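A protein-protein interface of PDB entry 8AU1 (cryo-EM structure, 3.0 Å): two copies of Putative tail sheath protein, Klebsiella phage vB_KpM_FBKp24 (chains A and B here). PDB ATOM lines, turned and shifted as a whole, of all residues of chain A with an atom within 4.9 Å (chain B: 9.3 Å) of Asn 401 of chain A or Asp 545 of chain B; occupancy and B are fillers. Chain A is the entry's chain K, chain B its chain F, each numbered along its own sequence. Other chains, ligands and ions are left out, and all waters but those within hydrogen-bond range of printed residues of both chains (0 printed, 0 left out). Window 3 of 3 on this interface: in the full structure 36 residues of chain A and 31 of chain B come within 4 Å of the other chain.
The side-chain carboxylate of Asp 564 of chain B lies within salt-bridge range of the guanidinium group of Arg 407 of chain A (3.5 Å). The backbone NH of Asn 401 of chain A is in hydrogen-bond range of the side-chain carboxylate of Asp 545 of chain B, at 3.5 Å.
The backbone carbonyl oxygen of Asn 543 of chain B lies close to the side-chain amino group of Lys 546 of chain B. OD1 of Asp 564 of chain B sits at hydrogen-bond distance from NE2 of Gln 570 of chain B, at 3.2 Å. The side-chain amide oxygen (OD1) of Asn 401 of chain A sits at hydrogen-bond distance from the side-chain hydroxyl (OG1) of Thr 403 of chain A (2.6 Å).
Lys 546 of chain B touches Asn 401 of chain A. ND2 of Asn 404 of chain A touches OD2 of Asp 564 of chain B, at 3.7 Å. Arg 407 of chain A touches Leu 544 of chain B. OH of Tyr 408 of chain A touches OD2 of Asp 545 of chain B, at 3.7 Å.
Of chain B, only Asp 545 and Lys 546 come within 4 Å of Asn 401 of chain A. Asp 545 of chain B touches two residues of chain A. Of the printed residues of chain A, Asp 564 of chain B touches Asn 404 (3.7 Å) and Arg 407 (3.5 Å). Of the printed residues of chain A, Leu 544 of chain B touches Arg 407. Asn 542 of chain B touches none of the printed residues of chain A. The nearest printed residue of chain A that does not touch Lys 546 of chain B is Thr 403 of chain A (6.3 Å).
Hydrophobic or aromatic side chains of chain A within 4 Å of the printed part of chain B: Tyr 408. Hydrophobic or aromatic side chains of chain B that line the printed part of chain A: Leu 544. Among the printed residues, Asp or Glu carboxylates within 4 Å of a Lys or Arg side-chain nitrogen of the other chain: Arg 407 of chain A with Asp 564 of chain B (3.5 Å).
No position is printed for both chains.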
ATOM      1  N   LEU A 394     -19.747  -8.036 -28.973  1.00  0.00           N
ATOM      2  CA  LEU A 394     -19.291  -6.734 -28.505  1.00  0.00           C
ATOM      3  C   LEU A 394     -17.894  -6.784 -27.913  1.00  0.00           C
ATOM      4  O   LEU A 394     -17.139  -5.814 -28.043  1.00  0.00           O
ATOM      5  CB  LEU A 394     -20.253  -6.180 -27.452  1.00  0.00           C
ATOM      6  CG  LEU A 394     -21.515  -5.480 -27.950  1.00  0.00           C
ATOM      7  CD1 LEU A 394     -22.327  -4.986 -26.774  1.00  0.00           C
ATOM      8  CD2 LEU A 394     -21.184  -4.336 -28.883  1.00  0.00           C
ATOM      9  N   ALA A 399     -14.064  -4.721 -35.771  1.00  0.00           N
ATOM     10  CA  ALA A 399     -14.379  -3.479 -36.463  1.00  0.00           C
ATOM     11  C   ALA A 399     -14.303  -2.273 -35.531  1.00  0.00           C
ATOM     12  O   ALA A 399     -13.831  -1.205 -35.932  1.00  0.00           O
ATOM     13  CB  ALA A 399     -15.771  -3.574 -37.091  1.00  0.00           C
ATOM     14  N   PHE A 400     -14.767  -2.425 -34.293  1.00  0.00           N
ATOM     15  CA  PHE A 400     -14.740  -1.333 -33.333  1.00  0.00           C
ATOM     16  C   PHE A 400     -15.113  -1.861 -31.956  1.00  0.00           C
ATOM     17  O   PHE A 400     -15.922  -2.783 -31.838  1.00  0.00           O
ATOM     18  CB  PHE A 400     -15.680  -0.199 -33.762  1.00  0.00           C
ATOM     19  CG  PHE A 400     -17.056  -0.661 -34.157  1.00  0.00           C
ATOM     20  CD1 PHE A 400     -17.953  -1.123 -33.211  1.00  0.00           C
ATOM     21  CD2 PHE A 400     -17.448  -0.634 -35.486  1.00  0.00           C
ATOM     22  CE1 PHE A 400     -19.211  -1.549 -33.583  1.00  0.00           C
ATOM     23  CE2 PHE A 400     -18.705  -1.055 -35.861  1.00  0.00           C
ATOM     24  CZ  PHE A 400     -19.586  -1.515 -34.910  1.00  0.00           C
ATOM     25  N   ASN A 401     -14.511  -1.273 -30.928  1.00  0.00           N
ATOM     26  CA  ASN A 401     -14.738  -1.654 -29.539  1.00  0.00           C
ATOM     27  C   ASN A 401     -15.476  -0.511 -28.853  1.00  0.00           C
ATOM     28  O   ASN A 401     -14.949   0.601 -28.759  1.00  0.00           O
ATOM     29  CB  ASN A 401     -13.407  -1.951 -28.854  1.00  0.00           C
ATOM     30  CG  ASN A 401     -13.514  -1.971 -27.350  1.00  0.00           C
ATOM     31  OD1 ASN A 401     -14.575  -2.245 -26.798  1.00  0.00           O
ATOM     32  ND2 ASN A 401     -12.406  -1.695 -26.675  1.00  0.00           N
ATOM     33  N   ILE A 402     -16.688  -0.781 -28.367  1.00  0.00           N
ATOM     34  CA  ILE A 402     -17.572   0.277 -27.886  1.00  0.00           C
ATOM     35  C   ILE A 402     -17.438   0.509 -26.385  1.00  0.00           C
ATOM     36  O   ILE A 402     -18.139   1.361 -25.836  1.00  0.00           O
ATOM     37  CB  ILE A 402     -19.038   0.004 -28.258  1.00  0.00           C
ATOM     38  CG1 ILE A 402     -19.577  -1.217 -27.517  1.00  0.00           C
ATOM     39  CG2 ILE A 402     -19.183  -0.170 -29.764  1.00  0.00           C
ATOM     40  CD1 ILE A 402     -21.066  -1.388 -27.674  1.00  0.00           C
ATOM     41  N   THR A 403     -16.550  -0.211 -25.711  1.00  0.00           N
ATOM     42  CA  THR A 403     -16.245   0.082 -24.319  1.00  0.00           C
ATOM     43  C   THR A 403     -15.276   1.246 -24.178  1.00  0.00           C
ATOM     44  O   THR A 403     -14.755   1.479 -23.083  1.00  0.00           O
ATOM     45  CB  THR A 403     -15.675  -1.154 -23.627  1.00  0.00           C
ATOM     46  OG1 THR A 403     -14.492  -1.584 -24.308  1.00  0.00           O
ATOM     47  CG2 THR A 403     -16.694  -2.276 -23.624  1.00  0.00           C
ATOM     48  N   ASN A 404     -15.026   1.975 -25.258  1.00  0.00           N
ATOM     49  CA  ASN A 404     -14.116   3.114 -25.263  1.00  0.00           C
ATOM     50  C   ASN A 404     -14.915   4.359 -24.905  1.00  0.00           C
ATOM     51  O   ASN A 404     -15.605   4.931 -25.749  1.00  0.00           O
ATOM     52  CB  ASN A 404     -13.463   3.240 -26.633  1.00  0.00           C
ATOM     53  CG  ASN A 404     -12.236   4.107 -26.620  1.00  0.00           C
ATOM     54  OD1 ASN A 404     -11.960   4.797 -25.643  1.00  0.00           O
ATOM     55  ND2 ASN A 404     -11.487   4.081 -27.712  1.00  0.00           N
ATOM     56  N   ARG A 407     -13.848   7.629 -26.934  1.00  0.00           N
ATOM     57  CA  ARG A 407     -13.979   7.608 -28.382  1.00  0.00           C
ATOM     58  C   ARG A 407     -15.408   7.416 -28.858  1.00  0.00           C
ATOM     59  O   ARG A 407     -15.697   7.704 -30.022  1.00  0.00           O
ATOM     60  CB  ARG A 407     -13.104   6.499 -28.963  1.00  0.00           C
ATOM     61  CG  ARG A 407     -12.920   6.603 -30.448  1.00  0.00           C
ATOM     62  CD  ARG A 407     -11.846   5.672 -30.940  1.00  0.00           C
ATOM     63  NE  ARG A 407     -11.827   5.623 -32.396  1.00  0.00           N
ATOM     64  CZ  ARG A 407     -10.838   6.060 -33.161  1.00  0.00           C
ATOM     65  NH1 ARG A 407      -9.770   6.647 -32.650  1.00  0.00           N
ATOM     66  NH2 ARG A 407     -10.931   5.920 -34.478  1.00  0.00           N
ATOM     67  N   TYR A 408     -16.302   6.931 -27.999  1.00  0.00           N
ATOM     68  CA  TYR A 408     -17.700   6.691 -28.351  1.00  0.00           C
ATOM     69  C   TYR A 408     -18.582   7.284 -27.262  1.00  0.00           C
ATOM     70  O   TYR A 408     -19.017   6.575 -26.347  1.00  0.00           O
ATOM     71  CB  TYR A 408     -17.955   5.199 -28.555  1.00  0.00           C
ATOM     72  CG  TYR A 408     -17.116   4.619 -29.673  1.00  0.00           C
ATOM     73  CD1 TYR A 408     -17.132   5.191 -30.934  1.00  0.00           C
ATOM     74  CD2 TYR A 408     -16.305   3.518 -29.470  1.00  0.00           C
ATOM     75  CE1 TYR A 408     -16.373   4.687 -31.955  1.00  0.00           C
ATOM     76  CE2 TYR A 408     -15.540   3.003 -30.492  1.00  0.00           C
ATOM     77  CZ  TYR A 408     -15.582   3.596 -31.731  1.00  0.00           C
ATOM     78  OH  TYR A 408     -14.825   3.093 -32.758  1.00  0.00           O
ATOM     79  N   ASN B 452      -1.029  -5.376 -33.338  1.00  0.00           N
ATOM     80  CA  ASN B 452      -0.737  -5.500 -31.913  1.00  0.00           C
ATOM     81  C   ASN B 452       0.346  -6.540 -31.660  1.00  0.00           C
ATOM     82  O   ASN B 452       1.255  -6.325 -30.850  1.00  0.00           O
ATOM     83  CB  ASN B 452      -2.009  -5.856 -31.147  1.00  0.00           C
ATOM     84  CG  ASN B 452      -3.047  -4.762 -31.204  1.00  0.00           C
ATOM     85  OD1 ASN B 452      -4.199  -5.002 -31.556  1.00  0.00           O
ATOM     86  ND2 ASN B 452      -2.648  -3.550 -30.851  1.00  0.00           N
ATOM     87  N   ILE B 541      -3.879   8.159 -35.830  1.00  0.00           N
ATOM     88  CA  ILE B 541      -3.081   7.147 -35.159  1.00  0.00           C
ATOM     89  C   ILE B 541      -3.793   5.803 -35.265  1.00  0.00           C
ATOM     90  O   ILE B 541      -5.015   5.732 -35.437  1.00  0.00           O
ATOM     91  CB  ILE B 541      -2.830   7.539 -33.693  1.00  0.00           C
ATOM     92  CG1 ILE B 541      -2.194   8.923 -33.611  1.00  0.00           C
ATOM     93  CG2 ILE B 541      -1.922   6.534 -33.019  1.00  0.00           C
ATOM     94  CD1 ILE B 541      -2.688   9.732 -32.453  1.00  0.00           C
ATOM     95  N   ASN B 542      -3.020   4.728 -35.172  1.00  0.00           N
ATOM     96  CA  ASN B 542      -3.512   3.382 -35.419  1.00  0.00           C
ATOM     97  C   ASN B 542      -3.683   2.605 -34.120  1.00  0.00           C
ATOM     98  O   ASN B 542      -3.159   2.976 -33.069  1.00  0.00           O
ATOM     99  CB  ASN B 542      -2.555   2.628 -36.345  1.00  0.00           C
ATOM    100  CG  ASN B 542      -1.177   2.476 -35.749  1.00  0.00           C
ATOM    101  OD1 ASN B 542      -0.504   3.461 -35.464  1.00  0.00           O
ATOM    102  ND2 ASN B 542      -0.752   1.238 -35.548  1.00  0.00           N
ATOM    103  N   ASN B 543      -4.436   1.508 -34.213  1.00  0.00           N
ATOM    104  CA  ASN B 543      -4.622   0.577 -33.100  1.00  0.00           C
ATOM    105  C   ASN B 543      -5.163   1.284 -31.864  1.00  0.00           C
ATOM    106  O   ASN B 543      -4.830   0.931 -30.734  1.00  0.00           O
ATOM    107  CB  ASN B 543      -3.320  -0.151 -32.764  1.00  0.00           C
ATOM    108  CG  ASN B 543      -2.804  -0.986 -33.911  1.00  0.00           C
ATOM    109  OD1 ASN B 543      -1.631  -0.909 -34.268  1.00  0.00           O
ATOM    110  ND2 ASN B 543      -3.677  -1.796 -34.493  1.00  0.00           N
ATOM    111  N   LEU B 544      -6.014   2.287 -32.073  1.00  0.00           N
ATOM    112  CA  LEU B 544      -6.561   3.016 -30.939  1.00  0.00           C
ATOM    113  C   LEU B 544      -7.626   2.219 -30.200  1.00  0.00           C
ATOM    114  O   LEU B 544      -7.965   2.569 -29.066  1.00  0.00           O
ATOM    115  CB  LEU B 544      -7.130   4.357 -31.397  1.00  0.00           C
ATOM    116  CG  LEU B 544      -6.097   5.477 -31.549  1.00  0.00           C
ATOM    117  CD1 LEU B 544      -6.725   6.689 -32.201  1.00  0.00           C
ATOM    118  CD2 LEU B 544      -5.494   5.855 -30.208  1.00  0.00           C
ATOM    119  N   ASP B 545      -8.164   1.168 -30.809  1.00  0.00           N
ATOM    120  CA  ASP B 545      -9.120   0.286 -30.139  1.00  0.00           C
ATOM    121  C   ASP B 545      -8.436  -0.933 -29.525  1.00  0.00           C
ATOM    122  O   ASP B 545      -8.832  -2.068 -29.776  1.00  0.00           O
ATOM    123  CB  ASP B 545     -10.201  -0.145 -31.123  1.00  0.00           C
ATOM    124  CG  ASP B 545     -11.055   1.006 -31.595  1.00  0.00           C
ATOM    125  OD1 ASP B 545     -10.670   1.671 -32.576  1.00  0.00           O
ATOM    126  OD2 ASP B 545     -12.119   1.242 -30.991  1.00  0.00           O
ATOM    127  N   LYS B 546      -7.410  -0.723 -28.706  1.00  0.00           N
ATOM    128  CA  LYS B 546      -6.764  -1.851 -28.053  1.00  0.00           C
ATOM    129  C   LYS B 546      -7.723  -2.501 -27.067  1.00  0.00           C
ATOM    130  O   LYS B 546      -8.682  -1.886 -26.601  1.00  0.00           O
ATOM    131  CB  LYS B 546      -5.506  -1.417 -27.305  1.00  0.00           C
ATOM    132  CG  LYS B 546      -4.449  -0.749 -28.142  1.00  0.00           C
ATOM    133  CD  LYS B 546      -3.358  -0.173 -27.253  1.00  0.00           C
ATOM    134  CE  LYS B 546      -2.621   0.962 -27.937  1.00  0.00           C
ATOM    135  NZ  LYS B 546      -3.391   2.234 -27.898  1.00  0.00           N
ATOM    136  N   SER B 547      -7.456  -3.760 -26.752  1.00  0.00           N
ATOM    137  CA  SER B 547      -8.175  -4.412 -25.676  1.00  0.00           C
ATOM    138  C   SER B 547      -7.562  -4.027 -24.336  1.00  0.00           C
ATOM    139  O   SER B 547      -6.409  -3.596 -24.247  1.00  0.00           O
ATOM    140  CB  SER B 547      -8.144  -5.926 -25.849  1.00  0.00           C
ATOM    141  OG  SER B 547      -8.809  -6.309 -27.038  1.00  0.00           O
ATOM    142  N   TRP B 548      -8.355  -4.187 -23.278  1.00  0.00           N
ATOM    143  CA  TRP B 548      -7.843  -3.927 -21.940  1.00  0.00           C
ATOM    144  C   TRP B 548      -6.634  -4.804 -21.653  1.00  0.00           C
ATOM    145  O   TRP B 548      -5.662  -4.363 -21.034  1.00  0.00           O
ATOM    146  CB  TRP B 548      -8.943  -4.162 -20.908  1.00  0.00           C
ATOM    147  CG  TRP B 548      -8.467  -4.101 -19.499  1.00  0.00           C
ATOM    148  CD1 TRP B 548      -8.637  -5.047 -18.539  1.00  0.00           C
ATOM    149  CD2 TRP B 548      -7.740  -3.033 -18.885  1.00  0.00           C
ATOM    150  NE1 TRP B 548      -8.066  -4.638 -17.362  1.00  0.00           N
ATOM    151  CE2 TRP B 548      -7.505  -3.404 -17.551  1.00  0.00           C
ATOM    152  CE3 TRP B 548      -7.262  -1.802 -19.336  1.00  0.00           C
ATOM    153  CZ2 TRP B 548      -6.816  -2.589 -16.664  1.00  0.00           C
ATOM    154  CZ3 TRP B 548      -6.580  -0.998 -18.458  1.00  0.00           C
ATOM    155  CH2 TRP B 548      -6.362  -1.392 -17.136  1.00  0.00           C
ATOM    156  N   ARG B 549      -6.672  -6.053 -22.116  1.00  0.00           N
ATOM    157  CA  ARG B 549      -5.547  -6.957 -21.907  1.00  0.00           C
ATOM    158  C   ARG B 549      -4.309  -6.477 -22.654  1.00  0.00           C
ATOM    159  O   ARG B 549      -3.191  -6.546 -22.133  1.00  0.00           O
ATOM    160  CB  ARG B 549      -5.932  -8.366 -22.347  1.00  0.00           C
ATOM    161  CG  ARG B 549      -6.777  -9.107 -21.327  1.00  0.00           C
ATOM    162  CD  ARG B 549      -8.243  -8.710 -21.418  1.00  0.00           C
ATOM    163  NE  ARG B 549      -8.851  -9.103 -22.685  1.00  0.00           N
ATOM    164  CZ  ARG B 549     -10.025  -8.666 -23.120  1.00  0.00           C
ATOM    165  NH1 ARG B 549     -10.745  -7.806 -22.417  1.00  0.00           N
ATOM    166  NH2 ARG B 549     -10.488  -9.101 -24.287  1.00  0.00           N
ATOM    167  N   VAL B 550      -4.486  -5.990 -23.881  1.00  0.00           N
ATOM    168  CA  VAL B 550      -3.351  -5.491 -24.650  1.00  0.00           C
ATOM    169  C   VAL B 550      -2.733  -4.287 -23.951  1.00  0.00           C
ATOM    170  O   VAL B 550      -1.505  -4.165 -23.844  1.00  0.00           O
ATOM    171  CB  VAL B 550      -3.783  -5.147 -26.085  1.00  0.00           C
ATOM    172  CG1 VAL B 550      -2.616  -4.579 -26.866  1.00  0.00           C
ATOM    173  CG2 VAL B 550      -4.341  -6.373 -26.776  1.00  0.00           C
ATOM    174  N   ARG B 551      -3.577  -3.374 -23.474  1.00  0.00           N
ATOM    175  CA  ARG B 551      -3.066  -2.206 -22.765  1.00  0.00           C
ATOM    176  C   ARG B 551      -2.347  -2.611 -21.486  1.00  0.00           C
ATOM    177  O   ARG B 551      -1.302  -2.049 -21.142  1.00  0.00           O
ATOM    178  CB  ARG B 551      -4.208  -1.242 -22.466  1.00  0.00           C
ATOM    179  CG  ARG B 551      -4.370  -0.174 -23.524  1.00  0.00           C
ATOM    180  CD  ARG B 551      -5.418   0.839 -23.143  1.00  0.00           C
ATOM    181  NE  ARG B 551      -6.761   0.296 -23.302  1.00  0.00           N
ATOM    182  CZ  ARG B 551      -7.762   0.478 -22.453  1.00  0.00           C
ATOM    183  NH1 ARG B 551      -7.617   1.196 -21.351  1.00  0.00           N
ATOM    184  NH2 ARG B 551      -8.942  -0.073 -22.717  1.00  0.00           N
ATOM    185  N   VAL B 562      -0.621   6.197 -26.425  1.00  0.00           N
ATOM    186  CA  VAL B 562      -1.604   7.258 -26.303  1.00  0.00           C
ATOM    187  C   VAL B 562      -2.994   6.650 -26.218  1.00  0.00           C
ATOM    188  O   VAL B 562      -3.242   5.521 -26.643  1.00  0.00           O
ATOM    189  CB  VAL B 562      -1.526   8.259 -27.475  1.00  0.00           C
ATOM    190  CG1 VAL B 562      -0.195   8.964 -27.480  1.00  0.00           C
ATOM    191  CG2 VAL B 562      -1.768   7.554 -28.795  1.00  0.00           C
ATOM    192  N   GLU B 563      -3.919   7.423 -25.663  1.00  0.00           N
ATOM    193  CA  GLU B 563      -5.328   7.080 -25.608  1.00  0.00           C
ATOM    194  C   GLU B 563      -6.129   8.240 -26.174  1.00  0.00           C
ATOM    195  O   GLU B 563      -5.589   9.309 -26.456  1.00  0.00           O
ATOM    196  CB  GLU B 563      -5.785   6.789 -24.180  1.00  0.00           C
ATOM    197  CG  GLU B 563      -5.255   5.500 -23.614  1.00  0.00           C
ATOM    198  CD  GLU B 563      -5.864   5.178 -22.270  1.00  0.00           C
ATOM    199  OE1 GLU B 563      -6.827   5.865 -21.880  1.00  0.00           O
ATOM    200  OE2 GLU B 563      -5.382   4.241 -21.602  1.00  0.00           O
ATOM    201  N   ASP B 564      -7.424   8.018 -26.349  1.00  0.00           N
ATOM    202  CA  ASP B 564      -8.294   9.079 -26.831  1.00  0.00           C
ATOM    203  C   ASP B 564      -8.663  10.019 -25.695  1.00  0.00           C
ATOM    204  O   ASP B 564      -9.233   9.599 -24.686  1.00  0.00           O
ATOM    205  CB  ASP B 564      -9.553   8.490 -27.451  1.00  0.00           C
ATOM    206  CG  ASP B 564      -9.292   7.858 -28.793  1.00  0.00           C
ATOM    207  OD1 ASP B 564      -9.327   8.582 -29.809  1.00  0.00           O
ATOM    208  OD2 ASP B 564      -9.031   6.640 -28.832  1.00  0.00           O
ATOM    209  N   GLN B 570      -5.922  12.881 -28.712  1.00  0.00           N
ATOM    210  CA  GLN B 570      -5.345  11.843 -27.869  1.00  0.00           C
ATOM    211  C   GLN B 570      -4.482  12.481 -26.790  1.00  0.00           C
ATOM    212  O   GLN B 570      -4.173  13.672 -26.844  1.00  0.00           O
ATOM    213  CB  GLN B 570      -4.500  10.867 -28.687  1.00  0.00           C
ATOM    214  CG  GLN B 570      -5.294   9.916 -29.553  1.00  0.00           C
ATOM    215  CD  GLN B 570      -5.778  10.558 -30.827  1.00  0.00           C
ATOM    216  OE1 GLN B 570      -5.131  11.449 -31.372  1.00  0.00           O
ATOM    217  NE2 GLN B 570      -6.915  10.097 -31.323  1.00  0.00           N
